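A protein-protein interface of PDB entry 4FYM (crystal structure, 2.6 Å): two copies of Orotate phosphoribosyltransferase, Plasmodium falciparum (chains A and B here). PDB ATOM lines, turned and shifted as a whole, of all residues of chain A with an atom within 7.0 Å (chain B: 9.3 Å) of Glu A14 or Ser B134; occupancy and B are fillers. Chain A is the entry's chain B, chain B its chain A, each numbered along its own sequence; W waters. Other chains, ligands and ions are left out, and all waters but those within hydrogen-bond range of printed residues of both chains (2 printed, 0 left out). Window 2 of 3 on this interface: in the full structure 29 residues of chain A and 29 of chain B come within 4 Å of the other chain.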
ATOM      1  N   LEU A  11      19.399 -33.743  23.974  1.00  0.00           N
ATOM      2  CA  LEU A  11      20.219 -33.510  22.815  1.00  0.00           C
ATOM      3  C   LEU A  11      21.207 -32.384  23.098  1.00  0.00           C
ATOM      4  O   LEU A  11      20.852 -31.390  23.706  1.00  0.00           O
ATOM      5  CB  LEU A  11      19.337 -33.043  21.641  1.00  0.00           C
ATOM      6  CG  LEU A  11      18.825 -34.018  20.579  1.00  0.00           C
ATOM      7  CD1 LEU A  11      18.443 -35.298  21.252  1.00  0.00           C
ATOM      8  CD2 LEU A  11      17.650 -33.387  19.848  1.00  0.00           C
ATOM      9  N   CYS A  12      22.410 -32.534  22.603  1.00  0.00           N
ATOM     10  CA  CYS A  12      23.406 -31.520  22.722  1.00  0.00           C
ATOM     11  C   CYS A  12      23.162 -30.435  21.634  1.00  0.00           C
ATOM     12  O   CYS A  12      22.525 -30.694  20.638  1.00  0.00           O
ATOM     13  CB  CYS A  12      24.810 -32.160  22.609  1.00  0.00           C
ATOM     14  SG  CYS A  12      25.279 -32.591  20.898  1.00  0.00           S
ATOM     15  N   ASP A  13      23.611 -29.221  21.909  1.00  0.00           N
ATOM     16  CA  ASP A  13      23.373 -28.099  21.033  1.00  0.00           C
ATOM     17  C   ASP A  13      23.822 -28.376  19.599  1.00  0.00           C
ATOM     18  O   ASP A  13      23.235 -27.856  18.671  1.00  0.00           O
ATOM     19  CB  ASP A  13      24.110 -26.855  21.546  1.00  0.00           C
ATOM     20  CG  ASP A  13      23.449 -26.198  22.761  1.00  0.00           C
ATOM     21  OD1 ASP A  13      22.275 -26.404  23.050  1.00  0.00           O
ATOM     22  OD2 ASP A  13      24.141 -25.397  23.401  1.00  0.00           O
ATOM     23  N   GLU A  14      24.894 -29.136  19.395  1.00  0.00           N
ATOM     24  CA  GLU A  14      25.381 -29.367  18.008  1.00  0.00           C
ATOM     25  C   GLU A  14      24.329 -30.191  17.257  1.00  0.00           C
ATOM     26  O   GLU A  14      24.060 -29.938  16.101  1.00  0.00           O
ATOM     27  CB  GLU A  14      26.753 -30.091  17.984  1.00  0.00           C
ATOM     28  CG  GLU A  14      27.994 -29.334  18.622  1.00  0.00           C
ATOM     29  CD  GLU A  14      28.183 -29.606  20.151  1.00  0.00           C
ATOM     30  OE1 GLU A  14      27.151 -29.572  20.930  1.00  0.00           O
ATOM     31  OE2 GLU A  14      29.369 -29.819  20.570  1.00  0.00           O
ATOM     32  N   GLU A  15      23.701 -31.134  17.951  1.00  0.00           N
ATOM     33  CA  GLU A  15      22.663 -31.994  17.340  1.00  0.00           C
ATOM     34  C   GLU A  15      21.389 -31.222  17.108  1.00  0.00           C
ATOM     35  O   GLU A  15      20.727 -31.409  16.086  1.00  0.00           O
ATOM     36  CB  GLU A  15      22.358 -33.223  18.209  1.00  0.00           C
ATOM     37  CG  GLU A  15      23.258 -34.476  18.001  1.00  0.00           C
ATOM     38  CD  GLU A  15      22.982 -35.566  19.135  1.00  0.00           C
ATOM     39  OE1 GLU A  15      23.118 -35.191  20.361  1.00  0.00           O
ATOM     40  OE2 GLU A  15      22.604 -36.793  18.852  1.00  0.00           O
ATOM     41  N   ILE A  16      21.053 -30.339  18.050  1.00  0.00           N
ATOM     42  CA  ILE A  16      19.878 -29.528  17.895  1.00  0.00           C
ATOM     43  C   ILE A  16      20.021 -28.701  16.622  1.00  0.00           C
ATOM     44  O   ILE A  16      19.064 -28.557  15.857  1.00  0.00           O
ATOM     45  CB  ILE A  16      19.633 -28.632  19.108  1.00  0.00           C
ATOM     46  CG1 ILE A  16      19.264 -29.469  20.301  1.00  0.00           C
ATOM     47  CG2 ILE A  16      18.498 -27.629  18.835  1.00  0.00           C
ATOM     48  CD1 ILE A  16      19.333 -28.719  21.601  1.00  0.00           C
ATOM     49  N   TYR A  17      21.178 -28.110  16.434  1.00  0.00           N
ATOM     50  CA  TYR A  17      21.375 -27.230  15.317  1.00  0.00           C
ATOM     51  C   TYR A  17      21.278 -28.015  14.010  1.00  0.00           C
ATOM     52  O   TYR A  17      20.551 -27.594  13.083  1.00  0.00           O
ATOM     53  CB  TYR A  17      22.710 -26.464  15.414  1.00  0.00           C
ATOM     54  CG  TYR A  17      22.952 -25.609  14.232  1.00  0.00           C
ATOM     55  CD1 TYR A  17      22.123 -24.540  13.958  1.00  0.00           C
ATOM     56  CD2 TYR A  17      23.962 -25.914  13.320  1.00  0.00           C
ATOM     57  CE1 TYR A  17      22.306 -23.780  12.809  1.00  0.00           C
ATOM     58  CE2 TYR A  17      24.179 -25.143  12.222  1.00  0.00           C
ATOM     59  CZ  TYR A  17      23.349 -24.074  11.983  1.00  0.00           C
ATOM     60  OH  TYR A  17      23.551 -23.330  10.850  1.00  0.00           O
ATOM     61  N   LYS A  18      21.944 -29.166  13.948  1.00  0.00           N
ATOM     62  CA  LYS A  18      21.880 -30.009  12.765  1.00  0.00           C
ATOM     63  C   LYS A  18      20.409 -30.328  12.433  1.00  0.00           C
ATOM     64  O   LYS A  18      20.010 -30.351  11.274  1.00  0.00           O
ATOM     65  CB  LYS A  18      22.653 -31.322  12.936  1.00  0.00           C
ATOM     66  CG  LYS A  18      24.140 -31.198  12.705  1.00  0.00           C
ATOM     67  CD  LYS A  18      24.909 -32.473  13.090  1.00  0.00           C
ATOM     68  CE  LYS A  18      26.408 -32.203  13.295  1.00  0.00           C
ATOM     69  NZ  LYS A  18      27.225 -33.344  12.809  1.00  0.00           N
ATOM     70  N   SER A  19      19.614 -30.600  13.433  1.00  0.00           N
ATOM     71  CA  SER A  19      18.240 -30.992  13.190  1.00  0.00           C
ATOM     72  C   SER A  19      17.390 -29.776  12.757  1.00  0.00           C
ATOM     73  O   SER A  19      16.616 -29.862  11.793  1.00  0.00           O
ATOM     74  CB  SER A  19      17.713 -31.615  14.456  1.00  0.00           C
ATOM     75  OG  SER A  19      16.350 -31.886  14.295  1.00  0.00           O
ATOM     76  N   LYS A  56      15.195 -28.553  27.829  1.00  0.00           N
ATOM     77  CA  LYS A  56      16.584 -28.536  28.081  1.00  0.00           C
ATOM     78  C   LYS A  56      17.068 -27.260  28.798  1.00  0.00           C
ATOM     79  O   LYS A  56      17.891 -27.337  29.671  1.00  0.00           O
ATOM     80  CB  LYS A  56      17.338 -28.687  26.757  1.00  0.00           C
ATOM     81  CG  LYS A  56      18.837 -28.616  26.892  1.00  0.00           C
ATOM     82  CD  LYS A  56      19.540 -28.608  25.555  1.00  0.00           C
ATOM     83  CE  LYS A  56      21.046 -28.567  25.863  1.00  0.00           C
ATOM     84  NZ  LYS A  56      21.887 -29.069  24.782  1.00  0.00           N
ATOM     85  N   TYR A  57      16.589 -26.096  28.391  1.00  0.00           N
ATOM     86  CA  TYR A  57      17.021 -24.853  28.948  1.00  0.00           C
ATOM     87  C   TYR A  57      16.144 -24.436  30.089  1.00  0.00           C
ATOM     88  O   TYR A  57      16.313 -23.366  30.684  1.00  0.00           O
ATOM     89  CB  TYR A  57      17.059 -23.800  27.849  1.00  0.00           C
ATOM     90  CG  TYR A  57      18.267 -23.981  27.012  1.00  0.00           C
ATOM     91  CD1 TYR A  57      19.514 -23.596  27.486  1.00  0.00           C
ATOM     92  CD2 TYR A  57      18.205 -24.593  25.767  1.00  0.00           C
ATOM     93  CE1 TYR A  57      20.654 -23.796  26.742  1.00  0.00           C
ATOM     94  CE2 TYR A  57      19.355 -24.773  24.984  1.00  0.00           C
ATOM     95  CZ  TYR A  57      20.579 -24.364  25.481  1.00  0.00           C
ATOM     96  OH  TYR A  57      21.763 -24.566  24.755  1.00  0.00           O
ATOM     97  N   ILE A  85      21.439 -18.464  20.616  1.00  0.00           N
ATOM     98  CA  ILE A  85      21.158 -18.502  19.190  1.00  0.00           C
ATOM     99  C   ILE A  85      20.610 -19.850  18.738  1.00  0.00           C
ATOM    100  O   ILE A  85      19.745 -19.885  17.852  1.00  0.00           O
ATOM    101  CB  ILE A  85      22.408 -18.091  18.370  1.00  0.00           C
ATOM    102  CG1 ILE A  85      22.054 -17.796  16.907  1.00  0.00           C
ATOM    103  CG2 ILE A  85      23.422 -19.176  18.359  1.00  0.00           C
ATOM    104  CD1 ILE A  85      21.158 -16.564  16.710  1.00  0.00           C
ATOM    105  N   VAL A  86      21.062 -20.948  19.350  1.00  0.00           N
ATOM    106  CA  VAL A  86      20.521 -22.215  18.959  1.00  0.00           C
ATOM    107  C   VAL A  86      19.016 -22.290  19.234  1.00  0.00           C
ATOM    108  O   VAL A  86      18.241 -22.826  18.416  1.00  0.00           O
ATOM    109  CB  VAL A  86      21.200 -23.362  19.704  1.00  0.00           C
ATOM    110  CG1 VAL A  86      20.424 -24.648  19.536  1.00  0.00           C
ATOM    111  CG2 VAL A  86      22.582 -23.553  19.171  1.00  0.00           C
ATOM    112  N   PHE B 106      34.770 -14.950  25.066  1.00  0.00           N
ATOM    113  CA  PHE B 106      33.588 -14.528  25.822  1.00  0.00           C
ATOM    114  C   PHE B 106      32.717 -15.716  26.150  1.00  0.00           C
ATOM    115  O   PHE B 106      32.702 -16.702  25.432  1.00  0.00           O
ATOM    116  CB  PHE B 106      32.750 -13.503  25.041  1.00  0.00           C
ATOM    117  CG  PHE B 106      32.206 -14.057  23.793  1.00  0.00           C
ATOM    118  CD1 PHE B 106      32.973 -14.100  22.645  1.00  0.00           C
ATOM    119  CD2 PHE B 106      30.978 -14.644  23.794  1.00  0.00           C
ATOM    120  CE1 PHE B 106      32.490 -14.677  21.486  1.00  0.00           C
ATOM    121  CE2 PHE B 106      30.476 -15.238  22.644  1.00  0.00           C
ATOM    122  CZ  PHE B 106      31.253 -15.259  21.496  1.00  0.00           C
ATOM    123  N   LEU B 127      28.279 -14.368  14.369  1.00  0.00           N
ATOM    124  CA  LEU B 127      29.332 -15.127  15.074  1.00  0.00           C
ATOM    125  C   LEU B 127      29.162 -16.585  14.931  1.00  0.00           C
ATOM    126  O   LEU B 127      30.102 -17.325  14.667  1.00  0.00           O
ATOM    127  CB  LEU B 127      29.324 -14.792  16.551  1.00  0.00           C
ATOM    128  CG  LEU B 127      30.218 -13.611  17.008  1.00  0.00           C
ATOM    129  CD1 LEU B 127      29.975 -13.253  18.447  1.00  0.00           C
ATOM    130  CD2 LEU B 127      31.688 -13.956  16.788  1.00  0.00           C
ATOM    131  N   PHE B 128      27.918 -17.037  15.057  1.00  0.00           N
ATOM    132  CA  PHE B 128      27.627 -18.479  15.005  1.00  0.00           C
ATOM    133  C   PHE B 128      28.002 -19.078  13.677  1.00  0.00           C
ATOM    134  O   PHE B 128      28.375 -20.235  13.614  1.00  0.00           O
ATOM    135  CB  PHE B 128      26.154 -18.731  15.289  1.00  0.00           C
ATOM    136  CG  PHE B 128      25.837 -20.138  15.612  1.00  0.00           C
ATOM    137  CD1 PHE B 128      26.333 -20.705  16.725  1.00  0.00           C
ATOM    138  CD2 PHE B 128      24.998 -20.885  14.793  1.00  0.00           C
ATOM    139  CE1 PHE B 128      26.080 -22.035  17.019  1.00  0.00           C
ATOM    140  CE2 PHE B 128      24.728 -22.210  15.064  1.00  0.00           C
ATOM    141  CZ  PHE B 128      25.258 -22.783  16.200  1.00  0.00           C
ATOM    142  N   GLU B 129      27.940 -18.297  12.615  1.00  0.00           N
ATOM    143  CA  GLU B 129      28.386 -18.796  11.283  1.00  0.00           C
ATOM    144  C   GLU B 129      29.856 -19.204  11.186  1.00  0.00           C
ATOM    145  O   GLU B 129      30.214 -19.951  10.324  1.00  0.00           O
ATOM    146  CB  GLU B 129      28.036 -17.777  10.192  1.00  0.00           C
ATOM    147  CG  GLU B 129      26.539 -17.768   9.985  1.00  0.00           C
ATOM    148  CD  GLU B 129      26.058 -16.814   8.932  1.00  0.00           C
ATOM    149  OE1 GLU B 129      26.829 -16.049   8.365  1.00  0.00           O
ATOM    150  OE2 GLU B 129      24.857 -16.842   8.663  1.00  0.00           O
ATOM    151  N   SER B 130      30.717 -18.698  12.077  1.00  0.00           N
ATOM    152  CA  SER B 130      32.124 -19.060  12.106  1.00  0.00           C
ATOM    153  C   SER B 130      32.367 -20.510  12.426  1.00  0.00           C
ATOM    154  O   SER B 130      33.483 -20.975  12.318  1.00  0.00           O
ATOM    155  CB  SER B 130      32.804 -18.259  13.181  1.00  0.00           C
ATOM    156  OG  SER B 130      32.528 -18.761  14.472  1.00  0.00           O
ATOM    157  N   LYS B 131      31.354 -21.203  12.938  1.00  0.00           N
ATOM    158  CA  LYS B 131      31.486 -22.594  13.354  1.00  0.00           C
ATOM    159  C   LYS B 131      32.450 -22.809  14.484  1.00  0.00           C
ATOM    160  O   LYS B 131      32.752 -23.934  14.830  1.00  0.00           O
ATOM    161  CB  LYS B 131      31.835 -23.490  12.189  1.00  0.00           C
ATOM    162  CG  LYS B 131      30.765 -23.436  11.119  1.00  0.00           C
ATOM    163  CD  LYS B 131      31.044 -24.396   9.970  1.00  0.00           C
ATOM    164  CE  LYS B 131      30.003 -24.194   8.879  1.00  0.00           C
ATOM    165  NZ  LYS B 131      30.183 -25.164   7.773  1.00  0.00           N
ATOM    166  N   LYS B 132      32.851 -21.762  15.159  1.00  0.00           N
ATOM    167  CA  LYS B 132      33.700 -21.955  16.334  1.00  0.00           C
ATOM    168  C   LYS B 132      32.937 -22.296  17.611  1.00  0.00           C
ATOM    169  O   LYS B 132      33.543 -22.497  18.655  1.00  0.00           O
ATOM    170  CB  LYS B 132      34.555 -20.688  16.578  1.00  0.00           C
ATOM    171  CG  LYS B 132      35.414 -20.260  15.389  1.00  0.00           C
ATOM    172  CD  LYS B 132      36.133 -18.870  15.504  1.00  0.00           C
ATOM    173  CE  LYS B 132      37.130 -18.770  16.727  1.00  0.00           C
ATOM    174  NZ  LYS B 132      38.540 -19.211  16.447  1.00  0.00           N
ATOM    175  N   TYR B 133      31.601 -22.251  17.578  1.00  0.00           N
ATOM    176  CA  TYR B 133      30.835 -22.198  18.824  1.00  0.00           C
ATOM    177  C   TYR B 133      29.710 -23.193  18.756  1.00  0.00           C
ATOM    178  O   TYR B 133      29.109 -23.372  17.730  1.00  0.00           O
ATOM    179  CB  TYR B 133      30.261 -20.807  19.063  1.00  0.00           C
ATOM    180  CG  TYR B 133      31.281 -19.674  18.974  1.00  0.00           C
ATOM    181  CD1 TYR B 133      32.022 -19.305  20.060  1.00  0.00           C
ATOM    182  CD2 TYR B 133      31.383 -18.899  17.837  1.00  0.00           C
ATOM    183  CE1 TYR B 133      32.899 -18.243  20.011  1.00  0.00           C
ATOM    184  CE2 TYR B 133      32.244 -17.841  17.764  1.00  0.00           C
ATOM    185  CZ  TYR B 133      32.995 -17.516  18.850  1.00  0.00           C
ATOM    186  OH  TYR B 133      33.897 -16.468  18.752  1.00  0.00           O
ATOM    187  N   SER B 134      29.434 -23.845  19.855  1.00  0.00           N
ATOM    188  CA  SER B 134      28.336 -24.770  19.861  1.00  0.00           C
ATOM    189  C   SER B 134      26.985 -24.015  20.121  1.00  0.00           C
ATOM    190  O   SER B 134      25.906 -24.488  19.761  1.00  0.00           O
ATOM    191  CB  SER B 134      28.580 -25.838  20.929  1.00  0.00           C
ATOM    192  OG  SER B 134      28.679 -25.239  22.215  1.00  0.00           O
ATOM    193  N   ASN B 135      27.097 -22.867  20.790  1.00  0.00           N
ATOM    194  CA  ASN B 135      26.000 -21.939  20.994  1.00  0.00           C
ATOM    195  C   ASN B 135      26.587 -20.554  21.283  1.00  0.00           C
ATOM    196  O   ASN B 135      27.803 -20.431  21.501  1.00  0.00           O
ATOM    197  CB  ASN B 135      25.151 -22.413  22.158  1.00  0.00           C
ATOM    198  CG  ASN B 135      23.698 -21.939  22.063  1.00  0.00           C
ATOM    199  OD1 ASN B 135      23.357 -21.009  21.322  1.00  0.00           O
ATOM    200  ND2 ASN B 135      22.841 -22.555  22.869  1.00  0.00           N
ATOM    201  N   ILE B 136      25.730 -19.524  21.254  1.00  0.00           N
ATOM    202  CA  ILE B 136      26.066 -18.195  21.711  1.00  0.00           C
ATOM    203  C   ILE B 136      24.978 -17.696  22.599  1.00  0.00           C
ATOM    204  O   ILE B 136      23.817 -17.649  22.215  1.00  0.00           O
ATOM    205  CB  ILE B 136      26.213 -17.271  20.555  1.00  0.00           C
ATOM    206  CG1 ILE B 136      27.395 -17.844  19.786  1.00  0.00           C
ATOM    207  CG2 ILE B 136      26.431 -15.838  21.004  1.00  0.00           C
ATOM    208  CD1 ILE B 136      28.069 -17.035  18.756  1.00  0.00           C
ATOM    209  N   PHE B 137      25.370 -17.311  23.797  1.00  0.00           N
ATOM    210  CA  PHE B 137      24.453 -16.895  24.814  1.00  0.00           C
ATOM    211  C   PHE B 137      24.492 -15.346  24.952  1.00  0.00           C
ATOM    212  O   PHE B 137      25.556 -14.760  25.082  1.00  0.00           O
ATOM    213  CB  PHE B 137      24.894 -17.544  26.097  1.00  0.00           C
ATOM    214  CG  PHE B 137      24.768 -18.998  26.060  1.00  0.00           C
ATOM    215  CD1 PHE B 137      23.543 -19.601  26.301  1.00  0.00           C
ATOM    216  CD2 PHE B 137      25.835 -19.806  25.823  1.00  0.00           C
ATOM    217  CE1 PHE B 137      23.391 -21.009  26.309  1.00  0.00           C
ATOM    218  CE2 PHE B 137      25.713 -21.191  25.857  1.00  0.00           C
ATOM    219  CZ  PHE B 137      24.474 -21.790  26.046  1.00  0.00           C
HETATM  220  O   HOH W   1      25.196 -25.848  17.628  1.00  0.00           O
HETATM  221  O   HOH W   2      26.717 -25.498  23.773  1.00  0.00           O
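The side-chain amide nitrogen (ND2) of Asn B135 is in hydrogen-bond range of the side-chain carboxylate (OD2) of Asp A13, 3.2 Å away.
The side-chain amide nitrogen of Asn B135 lies within hydrogen-bond range of the side-chain hydroxyl of Tyr A57 (3.0 Å).
The backbone NH of Ile A85 is in hydrogen-bond range of the side-chain amide oxygen of Asn B135.
OD1 of Asn B135 is in hydrogen-bond range of N of Val A86 (3.0 Å).
N of Ile A85 lies within hydrogen-bond range of O of Ile B136, 3.0 Å away.
The side-chain sulfur (SG) of Cys A12 sits at hydrogen-bond distance from the side-chain carboxylate (OE1) of Glu A14, 3.6 Å away.
OD1 of Asp A13 lies within salt-bridge range of NZ of Lys A56.
The side-chain hydroxyl (OH) of Tyr A57 is in hydrogen-bond range of the side-chain carboxylate (OD1) of Asp A13, 2.6 Å away.
O of Ser B134 touches CB of Asp A13, 3.5 Å away.
Ser B134 touches Glu A14.
CE1 of Tyr A17 touches CE2 of Phe B128 (3.7 Å).
Tyr A57 touches Phe B137 (CE1 to CE1, 3.9 Å).
CG2 of Ile A85 touches CD1 of Phe B128 (3.7 Å).
Ser B134 touches Val A86 (O to CG2, 3.5 Å).
Printed residues of chain A within 4 Å of Phe B137: Tyr A57.
Of the printed residues of chain B, Tyr A57 touches Asn B135 (3.0 Å) and Phe B137 (3.9 Å).
Printed residues of chain A within 4 Å of Phe B128: Tyr A17 (3.7 Å) and Ile A85 (3.7 Å).
Lys B132 touches none of the printed residues of chain A.
Cys A12 touches none of the printed residues of chain B.
The nearest residue of chain B that does not touch Glu A14 is Tyr B133 (6.1 Å).
The nearest residue of chain A that does not touch Ser B134 is Tyr A17 (5.7 Å).
The nearest printed residue of chain B that does not touch Ile A85 is Phe B137 (5.2 Å).
Of the 12 printed residues of chain B, 5 touch a printed residue of chain A.
Hydrophobic or aromatic side chains of chain B that line the printed part of chain A: Phe B128 and Phe B137.
Hydrophobic or aromatic side chains of chain A within 4 Å of the printed part of chain B: Tyr A17, Tyr A57, Ile A85 and Val A86.
Among the printed residues, 11 pairs touch across the chains.
Among the printed residues, no Asp or Glu carboxylate lies within 4 Å of a Lys or Arg side-chain nitrogen of the other chain.
No position is printed for both chains.
Water W2 lies within hydrogen-bond range of the side-chain hydroxyl of Ser B134 and the side-chain carboxylate of Asp A13.
Water W1 bridges the backbone carbonyl oxygen (O) of Ser B134 and the backbone carbonyl oxygen (O) of Asp A13.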
